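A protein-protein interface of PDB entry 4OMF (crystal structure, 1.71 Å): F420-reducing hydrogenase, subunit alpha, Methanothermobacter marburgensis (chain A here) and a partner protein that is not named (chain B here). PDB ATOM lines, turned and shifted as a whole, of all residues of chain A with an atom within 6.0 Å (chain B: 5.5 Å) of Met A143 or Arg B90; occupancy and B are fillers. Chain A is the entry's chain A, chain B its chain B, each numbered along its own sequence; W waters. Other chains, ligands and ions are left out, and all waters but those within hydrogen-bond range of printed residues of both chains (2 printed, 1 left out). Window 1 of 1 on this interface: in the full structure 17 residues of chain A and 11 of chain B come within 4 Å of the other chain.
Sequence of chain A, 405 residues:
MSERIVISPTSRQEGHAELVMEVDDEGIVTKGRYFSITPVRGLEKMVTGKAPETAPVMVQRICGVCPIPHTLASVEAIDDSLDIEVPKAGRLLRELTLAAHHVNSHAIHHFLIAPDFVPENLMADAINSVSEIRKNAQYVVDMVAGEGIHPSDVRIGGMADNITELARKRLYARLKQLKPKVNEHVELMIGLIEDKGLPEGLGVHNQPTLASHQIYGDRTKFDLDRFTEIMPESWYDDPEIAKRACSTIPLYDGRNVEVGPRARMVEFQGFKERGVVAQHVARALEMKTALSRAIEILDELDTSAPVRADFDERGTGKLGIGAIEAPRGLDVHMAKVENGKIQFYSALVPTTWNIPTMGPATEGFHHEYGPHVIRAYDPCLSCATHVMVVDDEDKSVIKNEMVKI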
ATOM      1  N   GLN A 138     -30.005   5.071  15.891  1.00  0.00           N
ATOM      2  CA  GLN A 138     -28.554   4.987  15.889  1.00  0.00           C
ATOM      3  C   GLN A 138     -27.989   3.658  16.428  1.00  0.00           C
ATOM      4  O   GLN A 138     -26.842   3.319  16.115  1.00  0.00           O
ATOM      5  CB  GLN A 138     -27.979   6.179  16.662  1.00  0.00           C
ATOM      6  CG  GLN A 138     -28.111   7.521  15.882  1.00  0.00           C
ATOM      7  CD  GLN A 138     -27.207   7.568  14.669  1.00  0.00           C
ATOM      8  OE1 GLN A 138     -27.480   6.936  13.642  1.00  0.00           O
ATOM      9  NE2 GLN A 138     -26.102   8.297  14.790  1.00  0.00           N
ATOM     10  N   TYR A 139     -28.761   2.887  17.205  1.00  0.00           N
ATOM     11  CA  TYR A 139     -28.321   1.514  17.495  1.00  0.00           C
ATOM     12  C   TYR A 139     -27.999   0.771  16.204  1.00  0.00           C
ATOM     13  O   TYR A 139     -27.042  -0.004  16.138  1.00  0.00           O
ATOM     14  CB  TYR A 139     -29.377   0.715  18.236  1.00  0.00           C
ATOM     15  CG  TYR A 139     -29.663   1.118  19.669  1.00  0.00           C
ATOM     16  CD1 TYR A 139     -28.631   1.341  20.583  1.00  0.00           C
ATOM     17  CD2 TYR A 139     -30.974   1.247  20.108  1.00  0.00           C
ATOM     18  CE1 TYR A 139     -28.913   1.687  21.908  1.00  0.00           C
ATOM     19  CE2 TYR A 139     -31.262   1.602  21.400  1.00  0.00           C
ATOM     20  CZ  TYR A 139     -30.235   1.832  22.301  1.00  0.00           C
ATOM     21  OH  TYR A 139     -30.550   2.164  23.601  1.00  0.00           O
ATOM     22  N   VAL A 140     -28.839   0.956  15.199  1.00  0.00           N
ATOM     23  CA  VAL A 140     -28.621   0.278  13.911  1.00  0.00           C
ATOM     24  C   VAL A 140     -27.331   0.725  13.230  1.00  0.00           C
ATOM     25  O   VAL A 140     -26.501  -0.102  12.788  1.00  0.00           O
ATOM     26  CB  VAL A 140     -29.797   0.522  12.935  1.00  0.00           C
ATOM     27  CG1 VAL A 140     -29.535  -0.192  11.613  1.00  0.00           C
ATOM     28  CG2 VAL A 140     -31.118   0.013  13.514  1.00  0.00           C
ATOM     29  N   VAL A 141     -27.163   2.035  13.122  1.00  0.00           N
ATOM     30  CA  VAL A 141     -26.003   2.552  12.408  1.00  0.00           C
ATOM     31  C   VAL A 141     -24.693   2.180  13.127  1.00  0.00           C
ATOM     32  O   VAL A 141     -23.747   1.772  12.465  1.00  0.00           O
ATOM     33  CB  VAL A 141     -26.068   4.069  12.218  1.00  0.00           C
ATOM     34  CG1 VAL A 141     -24.874   4.538  11.393  1.00  0.00           C
ATOM     35  CG2 VAL A 141     -27.401   4.466  11.501  1.00  0.00           C
ATOM     36  N   ASP A 142     -24.646   2.301  14.457  1.00  0.00           N
ATOM     37  CA  ASP A 142     -23.475   1.840  15.231  1.00  0.00           C
ATOM     38  C   ASP A 142     -23.206   0.326  15.035  1.00  0.00           C
ATOM     39  O   ASP A 142     -22.089  -0.067  14.660  1.00  0.00           O
ATOM     40  CB  ASP A 142     -23.642   2.120  16.732  1.00  0.00           C
ATOM     41  CG  ASP A 142     -23.204   3.535  17.148  1.00  0.00           C
ATOM     42  OD1 ASP A 142     -22.076   3.977  16.798  1.00  0.00           O
ATOM     43  OD2 ASP A 142     -24.010   4.201  17.841  1.00  0.00           O
ATOM     44  N   MET A 143     -24.195  -0.531  15.290  1.00  0.00           N
ATOM     45  CA  MET A 143     -23.925  -1.981  15.242  1.00  0.00           C
ATOM     46  C   MET A 143     -23.613  -2.493  13.841  1.00  0.00           C
ATOM     47  O   MET A 143     -22.722  -3.329  13.670  1.00  0.00           O
ATOM     48  CB  MET A 143     -25.092  -2.796  15.826  1.00  0.00           C
ATOM     49  CG  MET A 143     -25.267  -2.622  17.335  1.00  0.00           C
ATOM     50  SD  MET A 143     -26.539  -3.765  17.900  1.00  0.00           S
ATOM     51  CE  MET A 143     -26.758  -3.179  19.582  1.00  0.00           C
ATOM     52  N   VAL A 144     -24.319  -1.985  12.837  1.00  0.00           N
ATOM     53  CA  VAL A 144     -24.146  -2.499  11.481  1.00  0.00           C
ATOM     54  C   VAL A 144     -22.945  -1.870  10.793  1.00  0.00           C
ATOM     55  O   VAL A 144     -22.190  -2.553  10.111  1.00  0.00           O
ATOM     56  CB  VAL A 144     -25.396  -2.239  10.635  1.00  0.00           C
ATOM     57  CG1 VAL A 144     -25.157  -2.561   9.134  1.00  0.00           C
ATOM     58  CG2 VAL A 144     -26.599  -3.029  11.184  1.00  0.00           C
ATOM     59  N   ALA A 145     -22.788  -0.563  10.959  1.00  0.00           N
ATOM     60  CA  ALA A 145     -21.828   0.174  10.149  1.00  0.00           C
ATOM     61  C   ALA A 145     -20.609   0.704  10.923  1.00  0.00           C
ATOM     62  O   ALA A 145     -19.759   1.374  10.348  1.00  0.00           O
ATOM     63  CB  ALA A 145     -22.550   1.309   9.443  1.00  0.00           C
ATOM     64  N   GLY A 146     -20.502   0.396  12.216  1.00  0.00           N
ATOM     65  CA  GLY A 146     -19.256   0.632  12.920  1.00  0.00           C
ATOM     66  C   GLY A 146     -19.171   1.868  13.801  1.00  0.00           C
ATOM     67  O   GLY A 146     -18.529   1.825  14.838  1.00  0.00           O
ATOM     68  N   GLU A 147     -19.793   2.965  13.372  1.00  0.00           N
ATOM     69  CA  GLU A 147     -19.857   4.225  14.158  1.00  0.00           C
ATOM     70  C   GLU A 147     -21.122   4.956  13.710  1.00  0.00           C
ATOM     71  O   GLU A 147     -21.402   4.977  12.525  1.00  0.00           O
ATOM     72  CB  GLU A 147     -18.665   5.157  13.916  1.00  0.00           C
ATOM     73  CG  GLU A 147     -17.227   4.622  14.090  1.00  0.00           C
ATOM     74  CD  GLU A 147     -16.830   4.346  15.534  1.00  0.00           C
ATOM     75  OE1 GLU A 147     -17.493   4.850  16.476  1.00  0.00           O
ATOM     76  OE2 GLU A 147     -15.824   3.624  15.715  1.00  0.00           O
ATOM     77  N   GLY A 148     -21.839   5.595  14.635  1.00  0.00           N
ATOM     78  CA  GLY A 148     -23.088   6.248  14.298  1.00  0.00           C
ATOM     79  C   GLY A 148     -22.905   7.564  13.543  1.00  0.00           C
ATOM     80  O   GLY A 148     -23.826   8.051  12.895  1.00  0.00           O
ATOM     81  N   ASP A 153     -17.522   0.949   8.526  1.00  0.00           N
ATOM     82  CA  ASP A 153     -17.601  -0.405   7.987  1.00  0.00           C
ATOM     83  C   ASP A 153     -18.476  -0.603   6.752  1.00  0.00           C
ATOM     84  O   ASP A 153     -18.706  -1.750   6.334  1.00  0.00           O
ATOM     85  CB  ASP A 153     -18.028  -1.347   9.095  1.00  0.00           C
ATOM     86  CG  ASP A 153     -16.996  -1.395  10.230  1.00  0.00           C
ATOM     87  OD1 ASP A 153     -15.796  -1.061   9.981  1.00  0.00           O
ATOM     88  OD2 ASP A 153     -17.386  -1.736  11.367  1.00  0.00           O
ATOM     89  N   ILE A 163     -23.525  -9.075  11.038  1.00  0.00           N
ATOM     90  CA  ILE A 163     -23.812  -8.909  12.462  1.00  0.00           C
ATOM     91  C   ILE A 163     -24.247 -10.253  13.049  1.00  0.00           C
ATOM     92  O   ILE A 163     -24.500 -11.203  12.320  1.00  0.00           O
ATOM     93  CB  ILE A 163     -24.897  -7.835  12.701  1.00  0.00           C
ATOM     94  CG1 ILE A 163     -26.226  -8.242  12.058  1.00  0.00           C
ATOM     95  CG2 ILE A 163     -24.462  -6.484  12.139  1.00  0.00           C
ATOM     96  CD1 ILE A 163     -27.366  -7.237  12.333  1.00  0.00           C
ATOM     97  N   ALA A 167     -27.347  -9.236  17.715  1.00  0.00           N
ATOM     98  CA  ALA A 167     -27.530  -7.912  17.161  1.00  0.00           C
ATOM     99  C   ALA A 167     -28.822  -7.816  16.341  1.00  0.00           C
ATOM    100  O   ALA A 167     -29.618  -6.877  16.512  1.00  0.00           O
ATOM    101  CB  ALA A 167     -26.287  -7.515  16.288  1.00  0.00           C
ATOM    102  N   ARG A 170     -31.978  -7.962  18.453  1.00  0.00           N
ATOM    103  CA  ARG A 170     -32.053  -6.831  19.374  1.00  0.00           C
ATOM    104  C   ARG A 170     -32.541  -5.598  18.625  1.00  0.00           C
ATOM    105  O   ARG A 170     -33.461  -4.876  19.083  1.00  0.00           O
ATOM    106  CB  ARG A 170     -30.681  -6.606  20.013  1.00  0.00           C
ATOM    107  CG  ARG A 170     -30.439  -5.255  20.682  1.00  0.00           C
ATOM    108  CD  ARG A 170     -29.240  -5.375  21.616  1.00  0.00           C
ATOM    109  NE  ARG A 170     -29.603  -6.117  22.825  1.00  0.00           N
ATOM    110  CZ  ARG A 170     -28.738  -6.735  23.629  1.00  0.00           C
ATOM    111  NH1 ARG A 170     -29.174  -7.377  24.716  1.00  0.00           N
ATOM    112  NH2 ARG A 170     -27.432  -6.741  23.341  1.00  0.00           N
ATOM    113  N   LEU A 171     -31.953  -5.373  17.455  1.00  0.00           N
ATOM    114  CA  LEU A 171     -32.331  -4.239  16.622  1.00  0.00           C
ATOM    115  C   LEU A 171     -33.762  -4.361  16.127  1.00  0.00           C
ATOM    116  O   LEU A 171     -34.510  -3.366  16.077  1.00  0.00           O
ATOM    117  CB  LEU A 171     -31.376  -4.107  15.439  1.00  0.00           C
ATOM    118  CG  LEU A 171     -29.915  -3.778  15.791  1.00  0.00           C
ATOM    119  CD1 LEU A 171     -29.016  -3.887  14.539  1.00  0.00           C
ATOM    120  CD2 LEU A 171     -29.848  -2.368  16.380  1.00  0.00           C
ATOM    121  N   ARG A 174     -36.217  -3.439  18.852  1.00  0.00           N
ATOM    122  CA  ARG A 174     -36.228  -2.025  19.226  1.00  0.00           C
ATOM    123  C   ARG A 174     -36.891  -1.151  18.152  1.00  0.00           C
ATOM    124  O   ARG A 174     -37.685  -0.273  18.488  1.00  0.00           O
ATOM    125  CB  ARG A 174     -34.814  -1.548  19.541  1.00  0.00           C
ATOM    126  CG  ARG A 174     -34.365  -2.124  20.887  1.00  0.00           C
ATOM    127  CD  ARG A 174     -32.957  -1.718  21.228  1.00  0.00           C
ATOM    128  NE  ARG A 174     -32.493  -2.423  22.420  1.00  0.00           N
ATOM    129  CZ  ARG A 174     -31.232  -2.396  22.848  1.00  0.00           C
ATOM    130  NH1 ARG A 174     -30.316  -1.678  22.187  1.00  0.00           N
ATOM    131  NH2 ARG A 174     -30.885  -3.092  23.928  1.00  0.00           N
ATOM    132  N   LYS B  86     -14.156  -2.801  20.858  1.00  0.00           N
ATOM    133  CA  LYS B  86     -15.192  -2.027  20.161  1.00  0.00           C
ATOM    134  C   LYS B  86     -15.945  -2.886  19.140  1.00  0.00           C
ATOM    135  O   LYS B  86     -17.160  -2.755  19.049  1.00  0.00           O
ATOM    136  CB  LYS B  86     -14.666  -0.768  19.469  1.00  0.00           C
ATOM    137  CG  LYS B  86     -15.872   0.140  19.007  1.00  0.00           C
ATOM    138  CD  LYS B  86     -15.486   1.170  17.979  1.00  0.00           C
ATOM    139  CE  LYS B  86     -14.578   2.207  18.592  1.00  0.00           C
ATOM    140  NZ  LYS B  86     -13.874   2.983  17.528  1.00  0.00           N
ATOM    141  N   LYS B  87     -15.262  -3.750  18.392  1.00  0.00           N
ATOM    142  CA  LYS B  87     -15.966  -4.676  17.505  1.00  0.00           C
ATOM    143  C   LYS B  87     -17.058  -5.443  18.298  1.00  0.00           C
ATOM    144  O   LYS B  87     -18.166  -5.712  17.805  1.00  0.00           O
ATOM    145  CB  LYS B  87     -14.995  -5.664  16.858  1.00  0.00           C
ATOM    146  CG  LYS B  87     -15.641  -6.577  15.824  1.00  0.00           C
ATOM    147  CD  LYS B  87     -15.748  -5.892  14.462  1.00  0.00           C
ATOM    148  CE  LYS B  87     -16.582  -6.698  13.447  1.00  0.00           C
ATOM    149  NZ  LYS B  87     -16.217  -8.136  13.390  1.00  0.00           N
ATOM    150  N   ALA B  88     -16.726  -5.796  19.530  1.00  0.00           N
ATOM    151  CA  ALA B  88     -17.628  -6.595  20.347  1.00  0.00           C
ATOM    152  C   ALA B  88     -18.943  -5.872  20.605  1.00  0.00           C
ATOM    153  O   ALA B  88     -19.989  -6.508  20.649  1.00  0.00           O
ATOM    154  CB  ALA B  88     -16.943  -6.979  21.670  1.00  0.00           C
ATOM    155  N   VAL B  89     -18.914  -4.544  20.694  1.00  0.00           N
ATOM    156  CA  VAL B  89     -20.157  -3.817  20.978  1.00  0.00           C
ATOM    157  C   VAL B  89     -20.786  -3.248  19.696  1.00  0.00           C
ATOM    158  O   VAL B  89     -21.874  -2.655  19.740  1.00  0.00           O
ATOM    159  CB  VAL B  89     -19.936  -2.695  22.007  1.00  0.00           C
ATOM    160  CG1 VAL B  89     -19.446  -3.284  23.361  1.00  0.00           C
ATOM    161  CG2 VAL B  89     -18.962  -1.632  21.480  1.00  0.00           C
ATOM    162  N   ARG B  90     -20.124  -3.432  18.555  1.00  0.00           N
ATOM    163  CA  ARG B  90     -20.738  -3.033  17.287  1.00  0.00           C
ATOM    164  C   ARG B  90     -21.391  -4.248  16.635  1.00  0.00           C
ATOM    165  O   ARG B  90     -22.490  -4.619  17.031  1.00  0.00           O
ATOM    166  CB  ARG B  90     -19.717  -2.354  16.380  1.00  0.00           C
ATOM    167  CG  ARG B  90     -19.095  -1.103  17.052  1.00  0.00           C
ATOM    168  CD  ARG B  90     -20.089   0.045  17.229  1.00  0.00           C
ATOM    169  NE  ARG B  90     -19.352   1.301  17.377  1.00  0.00           N
ATOM    170  CZ  ARG B  90     -19.246   1.986  18.514  1.00  0.00           C
ATOM    171  NH1 ARG B  90     -19.861   1.574  19.618  1.00  0.00           N
ATOM    172  NH2 ARG B  90     -18.539   3.104  18.534  1.00  0.00           N
ATOM    173  N   GLN B  91     -20.732  -4.886  15.662  1.00  0.00           N
ATOM    174  CA  GLN B  91     -21.418  -5.944  14.921  1.00  0.00           C
ATOM    175  C   GLN B  91     -21.775  -7.154  15.777  1.00  0.00           C
ATOM    176  O   GLN B  91     -22.719  -7.869  15.444  1.00  0.00           O
ATOM    177  CB  GLN B  91     -20.583  -6.405  13.711  1.00  0.00           C
ATOM    178  CG  GLN B  91     -20.564  -5.397  12.554  1.00  0.00           C
ATOM    179  CD  GLN B  91     -19.524  -4.299  12.718  1.00  0.00           C
ATOM    180  OE1 GLN B  91     -18.762  -4.267  13.686  1.00  0.00           O
ATOM    181  NE2 GLN B  91     -19.501  -3.380  11.766  1.00  0.00           N
ATOM    182  N   TYR B  92     -21.049  -7.414  16.861  1.00  0.00           N
ATOM    183  CA  TYR B  92     -21.440  -8.570  17.695  1.00  0.00           C
ATOM    184  C   TYR B  92     -22.687  -8.267  18.539  1.00  0.00           C
ATOM    185  O   TYR B  92     -23.343  -9.194  19.050  1.00  0.00           O
ATOM    186  CB  TYR B  92     -20.297  -9.023  18.603  1.00  0.00           C
ATOM    187  CG  TYR B  92     -19.205  -9.778  17.871  1.00  0.00           C
ATOM    188  CD1 TYR B  92     -19.220 -11.169  17.812  1.00  0.00           C
ATOM    189  CD2 TYR B  92     -18.165  -9.102  17.245  1.00  0.00           C
ATOM    190  CE1 TYR B  92     -18.219 -11.870  17.135  1.00  0.00           C
ATOM    191  CE2 TYR B  92     -17.158  -9.796  16.576  1.00  0.00           C
ATOM    192  CZ  TYR B  92     -17.199 -11.175  16.528  1.00  0.00           C
ATOM    193  OH  TYR B  92     -16.202 -11.850  15.866  1.00  0.00           O
ATOM    194  N   GLY B  93     -23.013  -6.981  18.679  1.00  0.00           N
ATOM    195  CA  GLY B  93     -24.275  -6.570  19.298  1.00  0.00           C
ATOM    196  C   GLY B  93     -24.287  -6.566  20.829  1.00  0.00           C
ATOM    197  O   GLY B  93     -25.347  -6.404  21.448  1.00  0.00           O
ATOM    198  N   ILE B  94     -23.113  -6.742  21.445  1.00  0.00           N
ATOM    199  CA  ILE B  94     -23.023  -6.944  22.889  1.00  0.00           C
ATOM    200  C   ILE B  94     -23.175  -5.632  23.664  1.00  0.00           C
ATOM    201  O   ILE B  94     -22.543  -4.634  23.324  1.00  0.00           O
ATOM    202  CB  ILE B  94     -21.679  -7.615  23.251  1.00  0.00           C
ATOM    203  CG1 ILE B  94     -21.623  -9.036  22.689  1.00  0.00           C
ATOM    204  CG2 ILE B  94     -21.391  -7.567  24.773  1.00  0.00           C
ATOM    205  CD1 ILE B  94     -20.156  -9.557  22.543  1.00  0.00           C
ATOM    206  N   GLU B  95     -24.038  -5.629  24.676  1.00  0.00           N
ATOM    207  CA  GLU B  95     -24.209  -4.441  25.517  1.00  0.00           C
ATOM    208  C   GLU B  95     -23.709  -4.659  26.941  1.00  0.00           C
ATOM    209  O   GLU B  95     -23.639  -3.712  27.735  1.00  0.00           O
ATOM    210  CB  GLU B  95     -25.676  -4.004  25.535  1.00  0.00           C
ATOM    211  CG  GLU B  95     -26.043  -3.348  24.194  1.00  0.00           C
ATOM    212  CD  GLU B  95     -27.506  -2.926  24.095  1.00  0.00           C
ATOM    213  OE1 GLU B  95     -28.348  -3.454  24.860  1.00  0.00           O
ATOM    214  OE2 GLU B  95     -27.800  -2.077  23.219  1.00  0.00           O
ATOM    215  N   VAL B 119     -13.969   7.306  21.674  1.00  0.00           N
ATOM    216  CA  VAL B 119     -14.593   5.981  21.859  1.00  0.00           C
ATOM    217  C   VAL B 119     -16.064   6.135  22.264  1.00  0.00           C
ATOM    218  O   VAL B 119     -16.389   6.457  23.413  1.00  0.00           O
ATOM    219  CB  VAL B 119     -13.817   5.142  22.904  1.00  0.00           C
ATOM    220  CG1 VAL B 119     -14.366   3.721  22.979  1.00  0.00           C
ATOM    221  CG2 VAL B 119     -12.320   5.093  22.526  1.00  0.00           C
ATOM    222  N   ARG B 120     -16.933   5.961  21.277  1.00  0.00           N
ATOM    223  CA  ARG B 120     -18.373   6.164  21.409  1.00  0.00           C
ATOM    224  C   ARG B 120     -19.094   4.908  21.903  1.00  0.00           C
ATOM    225  O   ARG B 120     -18.937   3.874  21.302  1.00  0.00           O
ATOM    226  CB  ARG B 120     -18.931   6.585  20.032  1.00  0.00           C
ATOM    227  CG  ARG B 120     -20.445   6.629  19.873  1.00  0.00           C
ATOM    228  CD  ARG B 120     -20.751   6.869  18.377  1.00  0.00           C
ATOM    229  NE  ARG B 120     -22.158   6.592  18.061  1.00  0.00           N
ATOM    230  CZ  ARG B 120     -23.093   7.512  17.835  1.00  0.00           C
ATOM    231  NH1 ARG B 120     -22.796   8.808  17.841  1.00  0.00           N
ATOM    232  NH2 ARG B 120     -24.337   7.122  17.575  1.00  0.00           N
ATOM    233  N   PHE B 121     -19.869   5.022  22.986  1.00  0.00           N
ATOM    234  CA  PHE B 121     -20.752   3.953  23.483  1.00  0.00           C
ATOM    235  C   PHE B 121     -20.045   2.598  23.647  1.00  0.00           C
ATOM    236  O   PHE B 121     -20.501   1.559  23.127  1.00  0.00           O
ATOM    237  CB  PHE B 121     -21.964   3.797  22.555  1.00  0.00           C
ATOM    238  CG  PHE B 121     -22.797   5.060  22.404  1.00  0.00           C
ATOM    239  CD1 PHE B 121     -22.826   6.021  23.405  1.00  0.00           C
ATOM    240  CD2 PHE B 121     -23.550   5.275  21.263  1.00  0.00           C
ATOM    241  CE1 PHE B 121     -23.599   7.180  23.272  1.00  0.00           C
ATOM    242  CE2 PHE B 121     -24.335   6.442  21.129  1.00  0.00           C
ATOM    243  CZ  PHE B 121     -24.349   7.384  22.141  1.00  0.00           C
ATOM    244  N   LEU B 122     -18.931   2.624  24.369  1.00  0.00           N
ATOM    245  CA  LEU B 122     -18.263   1.401  24.803  1.00  0.00           C
ATOM    246  C   LEU B 122     -18.065   1.382  26.315  1.00  0.00           C
ATOM    247  O   LEU B 122     -18.310   0.365  26.956  1.00  0.00           O
ATOM    248  CB  LEU B 122     -16.921   1.231  24.090  1.00  0.00           C
ATOM    249  CG  LEU B 122     -16.018   0.152  24.716  1.00  0.00           C
ATOM    250  CD1 LEU B 122     -16.716  -1.231  24.662  1.00  0.00           C
ATOM    251  CD2 LEU B 122     -14.714   0.102  23.983  1.00  0.00           C
ATOM    252  N   LYS B 125     -20.421  -0.252  28.760  1.00  0.00           N
ATOM    253  CA  LYS B 125     -20.792  -1.628  28.426  1.00  0.00           C
ATOM    254  C   LYS B 125     -19.881  -2.674  29.038  1.00  0.00           C
ATOM    255  O   LYS B 125     -20.215  -3.857  29.037  1.00  0.00           O
ATOM    256  CB  LYS B 125     -20.827  -1.789  26.899  1.00  0.00           C
ATOM    257  CG  LYS B 125     -22.032  -1.043  26.323  1.00  0.00           C
ATOM    258  CD  LYS B 125     -21.992  -0.921  24.820  1.00  0.00           C
ATOM    259  CE  LYS B 125     -23.107   0.019  24.317  1.00  0.00           C
ATOM    260  NZ  LYS B 125     -23.026   0.136  22.828  1.00  0.00           N
HETATM  261  O   HOH W   1     -16.779  -2.216  14.051  1.00  0.00           O
HETATM  262  O   HOH W   2     -20.329  -4.227   8.887  1.00  0.00           O
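NH2 of Arg A174 is in salt-bridge range of OE1 of Glu B95, 2.7 Å away.
The side-chain carboxylate of Asp A153 lies within hydrogen-bond range of the side-chain amide nitrogen of Gln B91 (2.7 Å).
The side-chain carboxylate of Glu A147 is in salt-bridge range of the guanidinium group of Arg B90, 2.9 Å away.
O of Gly A146 sits at hydrogen-bond distance from NE of Arg B90.
The side-chain carboxylate (OD1) of Asp A142 is in salt-bridge range of the guanidinium group (NE) of Arg B120, 2.9 Å away.
N of Gln B91 lies close to O of Met A143 (3.2 Å).
The backbone carbonyl oxygen (O) of Gly B93 sits at hydrogen-bond distance from the guanidinium group (NH2) of Arg A170 (2.8 Å).
The side-chain carboxylate (OE2) of Glu A147 lies within salt-bridge range of the side-chain amino group (NZ) of Lys B86 (2.7 Å).
The guanidinium group (NE) of Arg B90 lies within salt-bridge range of the side-chain carboxylate (OD1) of Asp A142 (3.9 Å).
OE1 of Glu B95 lies within salt-bridge range of NE of Arg A170 (3.6 Å).
The backbone carbonyl oxygen (O) of Val A144 sits at hydrogen-bond distance from the side-chain amide nitrogen (NE2) of Gln B91 (3.3 Å).
The backbone carbonyl oxygen (O) of Ala A145 lies within hydrogen-bond range of the backbone NH (N) of Asp A153 (2.9 Å).
NE2 of Gln A138 lies within hydrogen-bond range of O of Gly A148, at 3.0 Å.
O of Arg B120 is in hydrogen-bond range of NH2 of Arg B90 (2.9 Å).
The backbone NH (N) of Gly A148 lies within hydrogen-bond range of the side-chain carboxylate (OD1) of Asp A142 (2.7 Å).
The backbone carbonyl oxygen of Phe B121 sits at hydrogen-bond distance from the side-chain amino group of Lys B125 (2.9 Å).
NE2 of Gln A138 touches NH2 of Arg B120, 3.5 Å away.
Phe B121 touches Asp A142.
Arg B90 touches Met A143 (C to O, 3.4 Å).
Met A143 touches Gly B93.
Met A143 touches Glu B95 (CE to OE2, 3.9 Å).
Gly A146 touches Gln B91.
N of Gly A148 touches NE of Arg B120, at 3.6 Å.
O of Gln B91 touches CA of Ile A163, 3.3 Å away.
Ala A167 touches Gln B91 (CB to O, 3.7 Å).
Gly B93 touches Ala A167 (CA to CB, 3.7 Å).
Printed residues of chain B within 4 Å of Met A143: Arg B90, Gln B91, Gly B93 and Glu B95.
Of chain A, only Asp A142, Met A143, Gly A146 and Glu A147 come within 4 Å of Arg B90.
Of the printed residues of chain B, Asp A142 touches Arg B90 (3.3 Å), Arg B120 (2.9 Å) and Phe B121 (3.6 Å).
Printed residues of chain B within 4 Å of Val A144: Gln B91.
Of the printed residues of chain B, Gly A148 touches Arg B120.
Val A140 touches none of the printed residues of chain B.
Lys B125 touches none of the printed residues of chain A.
The nearest residue of chain B that does not touch Met A143 is Val B89 (4.2 Å).
Of the 17 printed residues of chain A, 12 touch a printed residue of chain B.
Hydrophobic or aromatic side chains of chain A within 4 Å of the printed part of chain B: Met A143, Ile A163 and Ala A167.
Hydrophobic or aromatic side chains of chain B within 4 Å of the printed part of chain A: Phe B121.
Among the printed residues, 21 pairs touch across the chains.
Among the printed residues, Asp or Glu carboxylates within 4 Å of a Lys or Arg side-chain nitrogen of the other chain: Asp A142 with Arg B90 (3.9 Å), Asp A142 with Arg B120 (2.9 Å), Glu A147 with Lys B86 (2.7 Å), Glu A147 with Arg B90 (2.9 Å), Arg A170 with Glu B95 (3.6 Å) and Arg A174 with Glu B95 (2.7 Å).
Water W2 lies within hydrogen-bond range of the backbone carbonyl oxygen of Val A144 (2.8 Å) and the side-chain amide nitrogen of Gln B91 (3.1 Å).
Water W1 bridges the side-chain carboxylate of Asp A153 (2.8 Å) and the side-chain amide oxygen of Gln B91 (2.9 Å).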
